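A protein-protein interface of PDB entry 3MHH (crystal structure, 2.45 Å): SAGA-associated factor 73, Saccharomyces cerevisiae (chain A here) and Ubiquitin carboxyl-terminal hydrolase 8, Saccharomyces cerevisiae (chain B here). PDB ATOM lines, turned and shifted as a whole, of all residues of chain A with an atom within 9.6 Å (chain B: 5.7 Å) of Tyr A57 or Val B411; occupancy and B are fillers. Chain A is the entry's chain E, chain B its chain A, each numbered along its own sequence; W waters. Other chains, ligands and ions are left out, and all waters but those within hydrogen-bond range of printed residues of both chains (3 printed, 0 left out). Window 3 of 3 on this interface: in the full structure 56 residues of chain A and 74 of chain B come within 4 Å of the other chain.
Hydrophobic or aromatic side chains of chain B that line the printed part of chain A: Leu B359, Val B411, Pro B412 and Ile B414. Among the printed residues, no Asp or Glu carboxylate lies within 4 Å of a Lys or Arg side-chain nitrogen of the other chain.
Printed residues of chain B within 4 Å of Tyr A57: Lys B358, Leu B359, Val B411, Pro B412 and Ile B414. Val B411 touches one residue of chain A. Lys B358 touches just these residues of chain A: Lys A55, Lys A56, Tyr A57, Phe A58 and Asn A59. Of chain A, only Ser A53 (3.6 Å) and Tyr A57 (3.7 Å) come within 4 Å of Pro B412. Printed residues of chain B within 4 Å of Ser A53: Pro B412 (3.6 Å). Printed residues of chain B within 4 Å of Lys A55: Lys B358. Of the printed residues of chain A, Leu B359 touches Tyr A57 (2.8 Å), Phe A58 (3.2 Å) and Asn A59 (3.8 Å). Of the printed residues of chain B, Phe A58 touches Lys B358, Leu B359, Pro B360 and Ile B414. Printed residues of chain B within 4 Å of Asn A59: Lys B358 and Leu B359. Pro A60 touches none of the printed residues of chain B. Met B393 touches none of the printed residues of chain A. The nearest residue of chain A that does not touch Val B411 is Ser A53 (7.1 Å). The nearest printed residue of chain B that does not touch Lys A55 is His B357 (7.4 Å).
Water W2 lies within hydrogen-bond range of the backbone carbonyl oxygen (O) of Lys A55 (2.5 Å), the backbone carbonyl oxygen (O) of Phe A58 (3.1 Å) and the side-chain amino group (NZ) of Lys B358 (3.4 Å). Water W1 lies within hydrogen-bond range of the side-chain amide nitrogen (ND2) of Asn A59 and the backbone carbonyl oxygen (O) of Leu B359. Water W3 lies within hydrogen-bond range of O of His B357 (3.0 Å) and O of Lys A56 (3.3 Å).
Pro B412 touches Ser A53 (CG to OG, 3.6 Å). Tyr A57 touches Lys B358 (O to CA, 3.5 Å). Val B411 touches Tyr A57 (CG2 to OH, 3.5 Å). CE2 of Tyr A57 touches CD of Pro B412, 3.7 Å away. Tyr A57 touches Ile B414 (CG to CD1, 3.98 Å). Phe A58 touches Leu B359. Phe A58 touches Pro B360. CZ of Phe A58 touches CG2 of Ile B414, at 3.99 Å. CB of Lys B358 touches OD1 of Asn A59, 3.8 Å away. Asn A59 touches Leu B359 (ND2 to O, 3.8 Å).
The side-chain amino group (NZ) of Lys B358 sits at hydrogen-bond distance from the backbone carbonyl oxygen (O) of Lys A55, at 3.0 Å. The backbone carbonyl oxygen of Lys A56 sits at hydrogen-bond distance from the side-chain amino group of Lys B358. O of Phe A58 is in hydrogen-bond range of NZ of Lys B358 (2.8 Å). N of Leu B359 is in hydrogen-bond range of O of Tyr A57, 2.8 Å away.
The backbone NH of Met B393 sits at hydrogen-bond distance from the backbone carbonyl oxygen of Ile B414 (2.9 Å). The backbone NH (N) of Ser A53 is in hydrogen-bond range of the side-chain amide oxygen (OD1) of Asn A50 (2.9 Å). The side-chain carboxylate (OE2) of Glu A52 is in salt-bridge range of the side-chain amino group (NZ) of Lys A55 (3.1 Å).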
ATOM      1  N   ASN A  50       3.993 -24.385  15.493  1.00  0.00           N
ATOM      2  CA  ASN A  50       3.702 -23.210  14.711  1.00  0.00           C
ATOM      3  C   ASN A  50       2.212 -22.991  14.492  1.00  0.00           C
ATOM      4  O   ASN A  50       1.509 -23.849  13.951  1.00  0.00           O
ATOM      5  CB  ASN A  50       4.403 -23.313  13.369  1.00  0.00           C
ATOM      6  CG  ASN A  50       4.159 -22.112  12.507  1.00  0.00           C
ATOM      7  OD1 ASN A  50       3.026 -21.854  12.089  1.00  0.00           O
ATOM      8  ND2 ASN A  50       5.213 -21.344  12.254  1.00  0.00           N
ATOM      9  N   ARG A  51       1.748 -21.804  14.849  1.00  0.00           N
ATOM     10  CA  ARG A  51       0.328 -21.504  14.812  1.00  0.00           C
ATOM     11  C   ARG A  51      -0.240 -21.713  13.424  1.00  0.00           C
ATOM     12  O   ARG A  51      -1.295 -22.327  13.277  1.00  0.00           O
ATOM     13  CB  ARG A  51       0.063 -20.080  15.280  1.00  0.00           C
ATOM     14  CG  ARG A  51      -1.406 -19.718  15.320  1.00  0.00           C
ATOM     15  CD  ARG A  51      -1.595 -18.296  15.813  1.00  0.00           C
ATOM     16  NE  ARG A  51      -2.997 -17.901  15.803  1.00  0.00           N
ATOM     17  CZ  ARG A  51      -3.882 -18.284  16.716  1.00  0.00           C
ATOM     18  NH1 ARG A  51      -3.513 -19.090  17.709  1.00  0.00           N
ATOM     19  NH2 ARG A  51      -5.145 -17.879  16.624  1.00  0.00           N
ATOM     20  N   GLU A  52       0.464 -21.230  12.403  1.00  0.00           N
ATOM     21  CA  GLU A  52      -0.050 -21.332  11.030  1.00  0.00           C
ATOM     22  C   GLU A  52      -0.049 -22.766  10.509  1.00  0.00           C
ATOM     23  O   GLU A  52      -0.967 -23.180   9.823  1.00  0.00           O
ATOM     24  CB  GLU A  52       0.706 -20.395  10.075  1.00  0.00           C
ATOM     25  CG  GLU A  52       0.266 -18.926  10.182  1.00  0.00           C
ATOM     26  CD  GLU A  52      -1.236 -18.727   9.933  1.00  0.00           C
ATOM     27  OE1 GLU A  52      -1.764 -19.273   8.935  1.00  0.00           O
ATOM     28  OE2 GLU A  52      -1.889 -18.019  10.742  1.00  0.00           O
ATOM     29  N   SER A  53       0.984 -23.527  10.837  1.00  0.00           N
ATOM     30  CA  SER A  53       0.999 -24.947  10.519  1.00  0.00           C
ATOM     31  C   SER A  53      -0.143 -25.664  11.258  1.00  0.00           C
ATOM     32  O   SER A  53      -0.751 -26.595  10.735  1.00  0.00           O
ATOM     33  CB  SER A  53       2.339 -25.558  10.929  1.00  0.00           C
ATOM     34  OG  SER A  53       3.406 -24.988  10.207  1.00  0.00           O
ATOM     35  N   LEU A  54      -0.416 -25.249  12.490  1.00  0.00           N
ATOM     36  CA  LEU A  54      -1.496 -25.862  13.256  1.00  0.00           C
ATOM     37  C   LEU A  54      -2.828 -25.624  12.561  1.00  0.00           C
ATOM     38  O   LEU A  54      -3.629 -26.543  12.410  1.00  0.00           O
ATOM     39  CB  LEU A  54      -1.540 -25.330  14.687  1.00  0.00           C
ATOM     40  CG  LEU A  54      -0.497 -25.879  15.666  1.00  0.00           C
ATOM     41  CD1 LEU A  54      -0.724 -25.258  17.047  1.00  0.00           C
ATOM     42  CD2 LEU A  54      -0.496 -27.426  15.750  1.00  0.00           C
ATOM     43  N   LYS A  55      -3.065 -24.388  12.136  1.00  0.00           N
ATOM     44  CA  LYS A  55      -4.284 -24.068  11.410  1.00  0.00           C
ATOM     45  C   LYS A  55      -4.396 -24.935  10.170  1.00  0.00           C
ATOM     46  O   LYS A  55      -5.457 -25.461   9.848  1.00  0.00           O
ATOM     47  CB  LYS A  55      -4.295 -22.607  10.992  1.00  0.00           C
ATOM     48  CG  LYS A  55      -4.634 -21.641  12.113  1.00  0.00           C
ATOM     49  CD  LYS A  55      -4.918 -20.257  11.547  1.00  0.00           C
ATOM     50  CE  LYS A  55      -4.942 -19.210  12.633  1.00  0.00           C
ATOM     51  NZ  LYS A  55      -4.739 -17.861  12.070  1.00  0.00           N
ATOM     52  N   LYS A  56      -3.280 -25.105   9.480  1.00  0.00           N
ATOM     53  CA  LYS A  56      -3.290 -25.841   8.228  1.00  0.00           C
ATOM     54  C   LYS A  56      -3.443 -27.361   8.416  1.00  0.00           C
ATOM     55  O   LYS A  56      -4.291 -27.986   7.784  1.00  0.00           O
ATOM     56  CB  LYS A  56      -2.021 -25.518   7.440  1.00  0.00           C
ATOM     57  CG  LYS A  56      -2.130 -25.803   5.961  1.00  0.00           C
ATOM     58  CD  LYS A  56      -1.140 -24.981   5.166  1.00  0.00           C
ATOM     59  CE  LYS A  56      -1.329 -25.219   3.666  1.00  0.00           C
ATOM     60  NZ  LYS A  56      -2.774 -25.337   3.274  1.00  0.00           N
ATOM     61  N   TYR A  57      -2.643 -27.952   9.295  1.00  0.00           N
ATOM     62  CA  TYR A  57      -2.505 -29.404   9.310  1.00  0.00           C
ATOM     63  C   TYR A  57      -3.234 -30.100  10.443  1.00  0.00           C
ATOM     64  O   TYR A  57      -3.318 -31.334  10.471  1.00  0.00           O
ATOM     65  CB  TYR A  57      -1.037 -29.794   9.320  1.00  0.00           C
ATOM     66  CG  TYR A  57      -0.306 -29.315   8.093  1.00  0.00           C
ATOM     67  CD1 TYR A  57      -0.431 -29.983   6.889  1.00  0.00           C
ATOM     68  CD2 TYR A  57       0.502 -28.191   8.136  1.00  0.00           C
ATOM     69  CE1 TYR A  57       0.238 -29.549   5.765  1.00  0.00           C
ATOM     70  CE2 TYR A  57       1.181 -27.757   7.017  1.00  0.00           C
ATOM     71  CZ  TYR A  57       1.039 -28.437   5.837  1.00  0.00           C
ATOM     72  OH  TYR A  57       1.702 -28.008   4.712  1.00  0.00           O
ATOM     73  N   PHE A  58      -3.781 -29.309  11.351  1.00  0.00           N
ATOM     74  CA  PHE A  58      -4.520 -29.843  12.465  1.00  0.00           C
ATOM     75  C   PHE A  58      -5.922 -29.281  12.477  1.00  0.00           C
ATOM     76  O   PHE A  58      -6.246 -28.394  11.687  1.00  0.00           O
ATOM     77  CB  PHE A  58      -3.786 -29.568  13.771  1.00  0.00           C
ATOM     78  CG  PHE A  58      -2.550 -30.405  13.942  1.00  0.00           C
ATOM     79  CD1 PHE A  58      -2.587 -31.574  14.679  1.00  0.00           C
ATOM     80  CD2 PHE A  58      -1.367 -30.052  13.315  1.00  0.00           C
ATOM     81  CE1 PHE A  58      -1.456 -32.356  14.822  1.00  0.00           C
ATOM     82  CE2 PHE A  58      -0.234 -30.844  13.440  1.00  0.00           C
ATOM     83  CZ  PHE A  58      -0.278 -31.990  14.203  1.00  0.00           C
ATOM     84  N   ASN A  59      -6.763 -29.859  13.328  1.00  0.00           N
ATOM     85  CA  ASN A  59      -8.151 -29.433  13.464  1.00  0.00           C
ATOM     86  C   ASN A  59      -8.265 -28.161  14.307  1.00  0.00           C
ATOM     87  O   ASN A  59      -7.533 -27.982  15.274  1.00  0.00           O
ATOM     88  CB  ASN A  59      -8.976 -30.555  14.085  1.00  0.00           C
ATOM     89  CG  ASN A  59      -9.038 -31.783  13.201  1.00  0.00           C
ATOM     90  OD1 ASN A  59      -9.643 -31.758  12.132  1.00  0.00           O
ATOM     91  ND2 ASN A  59      -8.415 -32.872  13.649  1.00  0.00           N
ATOM     92  N   PRO A  60      -9.189 -27.269  13.933  1.00  0.00           N
ATOM     93  CA  PRO A  60      -9.348 -26.003  14.645  1.00  0.00           C
ATOM     94  C   PRO A  60      -9.600 -26.181  16.135  1.00  0.00           C
ATOM     95  O   PRO A  60      -9.143 -25.362  16.941  1.00  0.00           O
ATOM     96  CB  PRO A  60     -10.577 -25.366  13.975  1.00  0.00           C
ATOM     97  CG  PRO A  60     -10.723 -26.063  12.657  1.00  0.00           C
ATOM     98  CD  PRO A  60     -10.178 -27.440  12.855  1.00  0.00           C
ATOM     99  N   ALA A  62      -8.630 -28.806  18.010  1.00  0.00           N
ATOM    100  CA  ALA A  62      -7.738 -29.808  18.573  1.00  0.00           C
ATOM    101  C   ALA A  62      -7.290 -29.444  19.988  1.00  0.00           C
ATOM    102  O   ALA A  62      -6.981 -28.296  20.263  1.00  0.00           O
ATOM    103  CB  ALA A  62      -6.529 -30.001  17.672  1.00  0.00           C
ATOM    104  N   LEU A  64      -4.355 -29.425  22.570  1.00  0.00           N
ATOM    105  CA  LEU A  64      -2.922 -29.417  22.406  1.00  0.00           C
ATOM    106  C   LEU A  64      -2.229 -29.251  23.744  1.00  0.00           C
ATOM    107  O   LEU A  64      -2.458 -28.280  24.452  1.00  0.00           O
ATOM    108  CB  LEU A  64      -2.514 -28.296  21.444  1.00  0.00           C
ATOM    109  CG  LEU A  64      -2.901 -28.504  19.979  1.00  0.00           C
ATOM    110  CD1 LEU A  64      -2.635 -27.248  19.171  1.00  0.00           C
ATOM    111  CD2 LEU A  64      -2.140 -29.696  19.381  1.00  0.00           C
ATOM    112  N   HIS B 357      -5.185 -35.282   5.318  1.00  0.00           N
ATOM    113  CA  HIS B 357      -5.743 -33.926   5.210  1.00  0.00           C
ATOM    114  C   HIS B 357      -5.582 -33.219   6.551  1.00  0.00           C
ATOM    115  O   HIS B 357      -5.110 -32.093   6.619  1.00  0.00           O
ATOM    116  CB  HIS B 357      -7.230 -33.988   4.790  1.00  0.00           C
ATOM    117  CG  HIS B 357      -7.900 -32.649   4.692  1.00  0.00           C
ATOM    118  ND1 HIS B 357      -7.449 -31.648   3.858  1.00  0.00           N
ATOM    119  CD2 HIS B 357      -8.984 -32.147   5.330  1.00  0.00           C
ATOM    120  CE1 HIS B 357      -8.213 -30.579   4.005  1.00  0.00           C
ATOM    121  NE2 HIS B 357      -9.157 -30.859   4.886  1.00  0.00           N
ATOM    122  N   LYS B 358      -5.953 -33.904   7.626  1.00  0.00           N
ATOM    123  CA  LYS B 358      -5.784 -33.377   8.972  1.00  0.00           C
ATOM    124  C   LYS B 358      -5.188 -34.431   9.888  1.00  0.00           C
ATOM    125  O   LYS B 358      -5.632 -35.573   9.894  1.00  0.00           O
ATOM    126  CB  LYS B 358      -7.119 -32.909   9.546  1.00  0.00           C
ATOM    127  CG  LYS B 358      -7.709 -31.676   8.860  1.00  0.00           C
ATOM    128  CD  LYS B 358      -6.869 -30.444   9.119  1.00  0.00           C
ATOM    129  CE  LYS B 358      -7.500 -29.204   8.518  1.00  0.00           C
ATOM    130  NZ  LYS B 358      -6.804 -27.976   9.025  1.00  0.00           N
ATOM    131  N   LEU B 359      -4.200 -34.021  10.682  1.00  0.00           N
ATOM    132  CA  LEU B 359      -3.565 -34.892  11.652  1.00  0.00           C
ATOM    133  C   LEU B 359      -4.217 -34.734  13.012  1.00  0.00           C
ATOM    134  O   LEU B 359      -4.699 -33.648  13.340  1.00  0.00           O
ATOM    135  CB  LEU B 359      -2.096 -34.520  11.810  1.00  0.00           C
ATOM    136  CG  LEU B 359      -1.104 -34.997  10.766  1.00  0.00           C
ATOM    137  CD1 LEU B 359       0.263 -34.336  11.031  1.00  0.00           C
ATOM    138  CD2 LEU B 359      -1.010 -36.500  10.821  1.00  0.00           C
ATOM    139  N   PRO B 360      -4.163 -35.789  13.836  1.00  0.00           N
ATOM    140  CA  PRO B 360      -4.652 -35.749  15.206  1.00  0.00           C
ATOM    141  C   PRO B 360      -3.549 -35.337  16.179  1.00  0.00           C
ATOM    142  O   PRO B 360      -2.381 -35.372  15.831  1.00  0.00           O
ATOM    143  CB  PRO B 360      -5.034 -37.202  15.460  1.00  0.00           C
ATOM    144  CG  PRO B 360      -3.996 -37.971  14.709  1.00  0.00           C
ATOM    145  CD  PRO B 360      -3.643 -37.123  13.493  1.00  0.00           C
ATOM    146  N   MET B 393       5.771 -36.863  10.289  1.00  0.00           N
ATOM    147  CA  MET B 393       4.648 -37.157   9.416  1.00  0.00           C
ATOM    148  C   MET B 393       4.593 -36.286   8.163  1.00  0.00           C
ATOM    149  O   MET B 393       3.657 -36.407   7.371  1.00  0.00           O
ATOM    150  CB  MET B 393       3.334 -37.034  10.193  1.00  0.00           C
ATOM    151  CG  MET B 393       3.082 -38.175  11.197  1.00  0.00           C
ATOM    152  SD  MET B 393       3.108 -39.773  10.394  1.00  0.00           S
ATOM    153  CE  MET B 393       1.694 -39.600   9.337  1.00  0.00           C
ATOM    154  N   LYS B 394       5.613 -35.464   7.936  1.00  0.00           N
ATOM    155  CA  LYS B 394       5.527 -34.447   6.902  1.00  0.00           C
ATOM    156  C   LYS B 394       5.367 -35.007   5.500  1.00  0.00           C
ATOM    157  O   LYS B 394       4.661 -34.428   4.674  1.00  0.00           O
ATOM    158  CB  LYS B 394       6.719 -33.485   6.969  1.00  0.00           C
ATOM    159  CG  LYS B 394       8.032 -34.014   6.427  1.00  0.00           C
ATOM    160  CD  LYS B 394       9.154 -33.008   6.665  1.00  0.00           C
ATOM    161  CE  LYS B 394      10.428 -33.358   5.891  1.00  0.00           C
ATOM    162  NZ  LYS B 394      11.629 -32.711   6.518  1.00  0.00           N
ATOM    163  N   ASN B 395       6.013 -36.138   5.230  1.00  0.00           N
ATOM    164  CA  ASN B 395       5.950 -36.754   3.900  1.00  0.00           C
ATOM    165  C   ASN B 395       4.580 -37.353   3.553  1.00  0.00           C
ATOM    166  O   ASN B 395       4.364 -37.793   2.436  1.00  0.00           O
ATOM    167  CB  ASN B 395       7.022 -37.849   3.775  1.00  0.00           C
ATOM    168  CG  ASN B 395       8.423 -37.288   3.540  1.00  0.00           C
ATOM    169  OD1 ASN B 395       8.587 -36.144   3.133  1.00  0.00           O
ATOM    170  ND2 ASN B 395       9.438 -38.111   3.781  1.00  0.00           N
ATOM    171  N   CYS B 397       1.411 -35.900   4.422  1.00  0.00           N
ATOM    172  CA  CYS B 397       0.327 -34.939   4.387  1.00  0.00           C
ATOM    173  C   CYS B 397       0.154 -34.518   2.929  1.00  0.00           C
ATOM    174  O   CYS B 397       1.135 -34.273   2.238  1.00  0.00           O
ATOM    175  CB  CYS B 397       0.661 -33.727   5.256  1.00  0.00           C
ATOM    176  SG  CYS B 397       0.759 -34.031   7.037  1.00  0.00           S
ATOM    177  N   SER B 398      -1.090 -34.475   2.464  1.00  0.00           N
ATOM    178  CA  SER B 398      -1.402 -34.035   1.109  1.00  0.00           C
ATOM    179  C   SER B 398      -0.900 -32.616   0.838  1.00  0.00           C
ATOM    180  O   SER B 398      -0.745 -31.812   1.767  1.00  0.00           O
ATOM    181  CB  SER B 398      -2.916 -34.100   0.879  1.00  0.00           C
ATOM    182  OG  SER B 398      -3.407 -35.413   1.116  1.00  0.00           O
ATOM    183  N   LYS B 410       6.094 -26.540   0.650  1.00  0.00           N
ATOM    184  CA  LYS B 410       6.680 -27.672   1.353  1.00  0.00           C
ATOM    185  C   LYS B 410       6.004 -27.854   2.717  1.00  0.00           C
ATOM    186  O   LYS B 410       5.802 -26.885   3.457  1.00  0.00           O
ATOM    187  CB  LYS B 410       8.190 -27.465   1.556  1.00  0.00           C
ATOM    188  CG  LYS B 410       8.932 -26.907   0.331  1.00  0.00           C
ATOM    189  CD  LYS B 410       9.004 -25.375   0.357  1.00  0.00           C
ATOM    190  CE  LYS B 410       9.241 -24.788  -1.031  1.00  0.00           C
ATOM    191  NZ  LYS B 410       9.163 -23.291  -1.053  1.00  0.00           N
ATOM    192  N   VAL B 411       5.675 -29.097   3.051  1.00  0.00           N
ATOM    193  CA  VAL B 411       5.145 -29.398   4.368  1.00  0.00           C
ATOM    194  C   VAL B 411       6.295 -29.369   5.383  1.00  0.00           C
ATOM    195  O   VAL B 411       7.361 -29.940   5.149  1.00  0.00           O
ATOM    196  CB  VAL B 411       4.403 -30.756   4.392  1.00  0.00           C
ATOM    197  CG1 VAL B 411       3.783 -30.996   5.751  1.00  0.00           C
ATOM    198  CG2 VAL B 411       3.327 -30.775   3.320  1.00  0.00           C
ATOM    199  N   PRO B 412       6.093 -28.661   6.502  1.00  0.00           N
ATOM    200  CA  PRO B 412       7.123 -28.556   7.527  1.00  0.00           C
ATOM    201  C   PRO B 412       7.278 -29.848   8.335  1.00  0.00           C
ATOM    202  O   PRO B 412       6.420 -30.740   8.265  1.00  0.00           O
ATOM    203  CB  PRO B 412       6.605 -27.422   8.417  1.00  0.00           C
ATOM    204  CG  PRO B 412       5.128 -27.488   8.275  1.00  0.00           C
ATOM    205  CD  PRO B 412       4.884 -27.891   6.850  1.00  0.00           C
ATOM    206  N   ASP B 413       8.369 -29.956   9.088  1.00  0.00           N
ATOM    207  CA  ASP B 413       8.511 -31.076   9.992  1.00  0.00           C
ATOM    208  C   ASP B 413       7.327 -31.056  10.943  1.00  0.00           C
ATOM    209  O   ASP B 413       7.028 -30.024  11.543  1.00  0.00           O
ATOM    210  CB  ASP B 413       9.803 -30.984  10.793  1.00  0.00           C
ATOM    211  CG  ASP B 413      11.030 -31.001   9.920  1.00  0.00           C
ATOM    212  OD1 ASP B 413      11.101 -31.837   8.978  1.00  0.00           O
ATOM    213  OD2 ASP B 413      11.924 -30.166  10.190  1.00  0.00           O
ATOM    214  N   ILE B 414       6.634 -32.187  11.027  1.00  0.00           N
ATOM    215  CA  ILE B 414       5.586 -32.422  12.011  1.00  0.00           C
ATOM    216  C   ILE B 414       5.941 -33.693  12.787  1.00  0.00           C
ATOM    217  O   ILE B 414       5.781 -34.810  12.289  1.00  0.00           O
ATOM    218  CB  ILE B 414       4.234 -32.608  11.339  1.00  0.00           C
ATOM    219  CG1 ILE B 414       3.872 -31.353  10.559  1.00  0.00           C
ATOM    220  CG2 ILE B 414       3.164 -32.884  12.388  1.00  0.00           C
ATOM    221  CD1 ILE B 414       2.602 -31.487   9.731  1.00  0.00           C
HETATM  222  O   HOH W   1      -6.286 -32.253  15.073  1.00  0.00           O
HETATM  223  O   HOH W   2      -7.417 -25.556  11.378  1.00  0.00           O
HETATM  224  O   HOH W   3      -4.219 -29.781   4.991  1.00  0.00           O
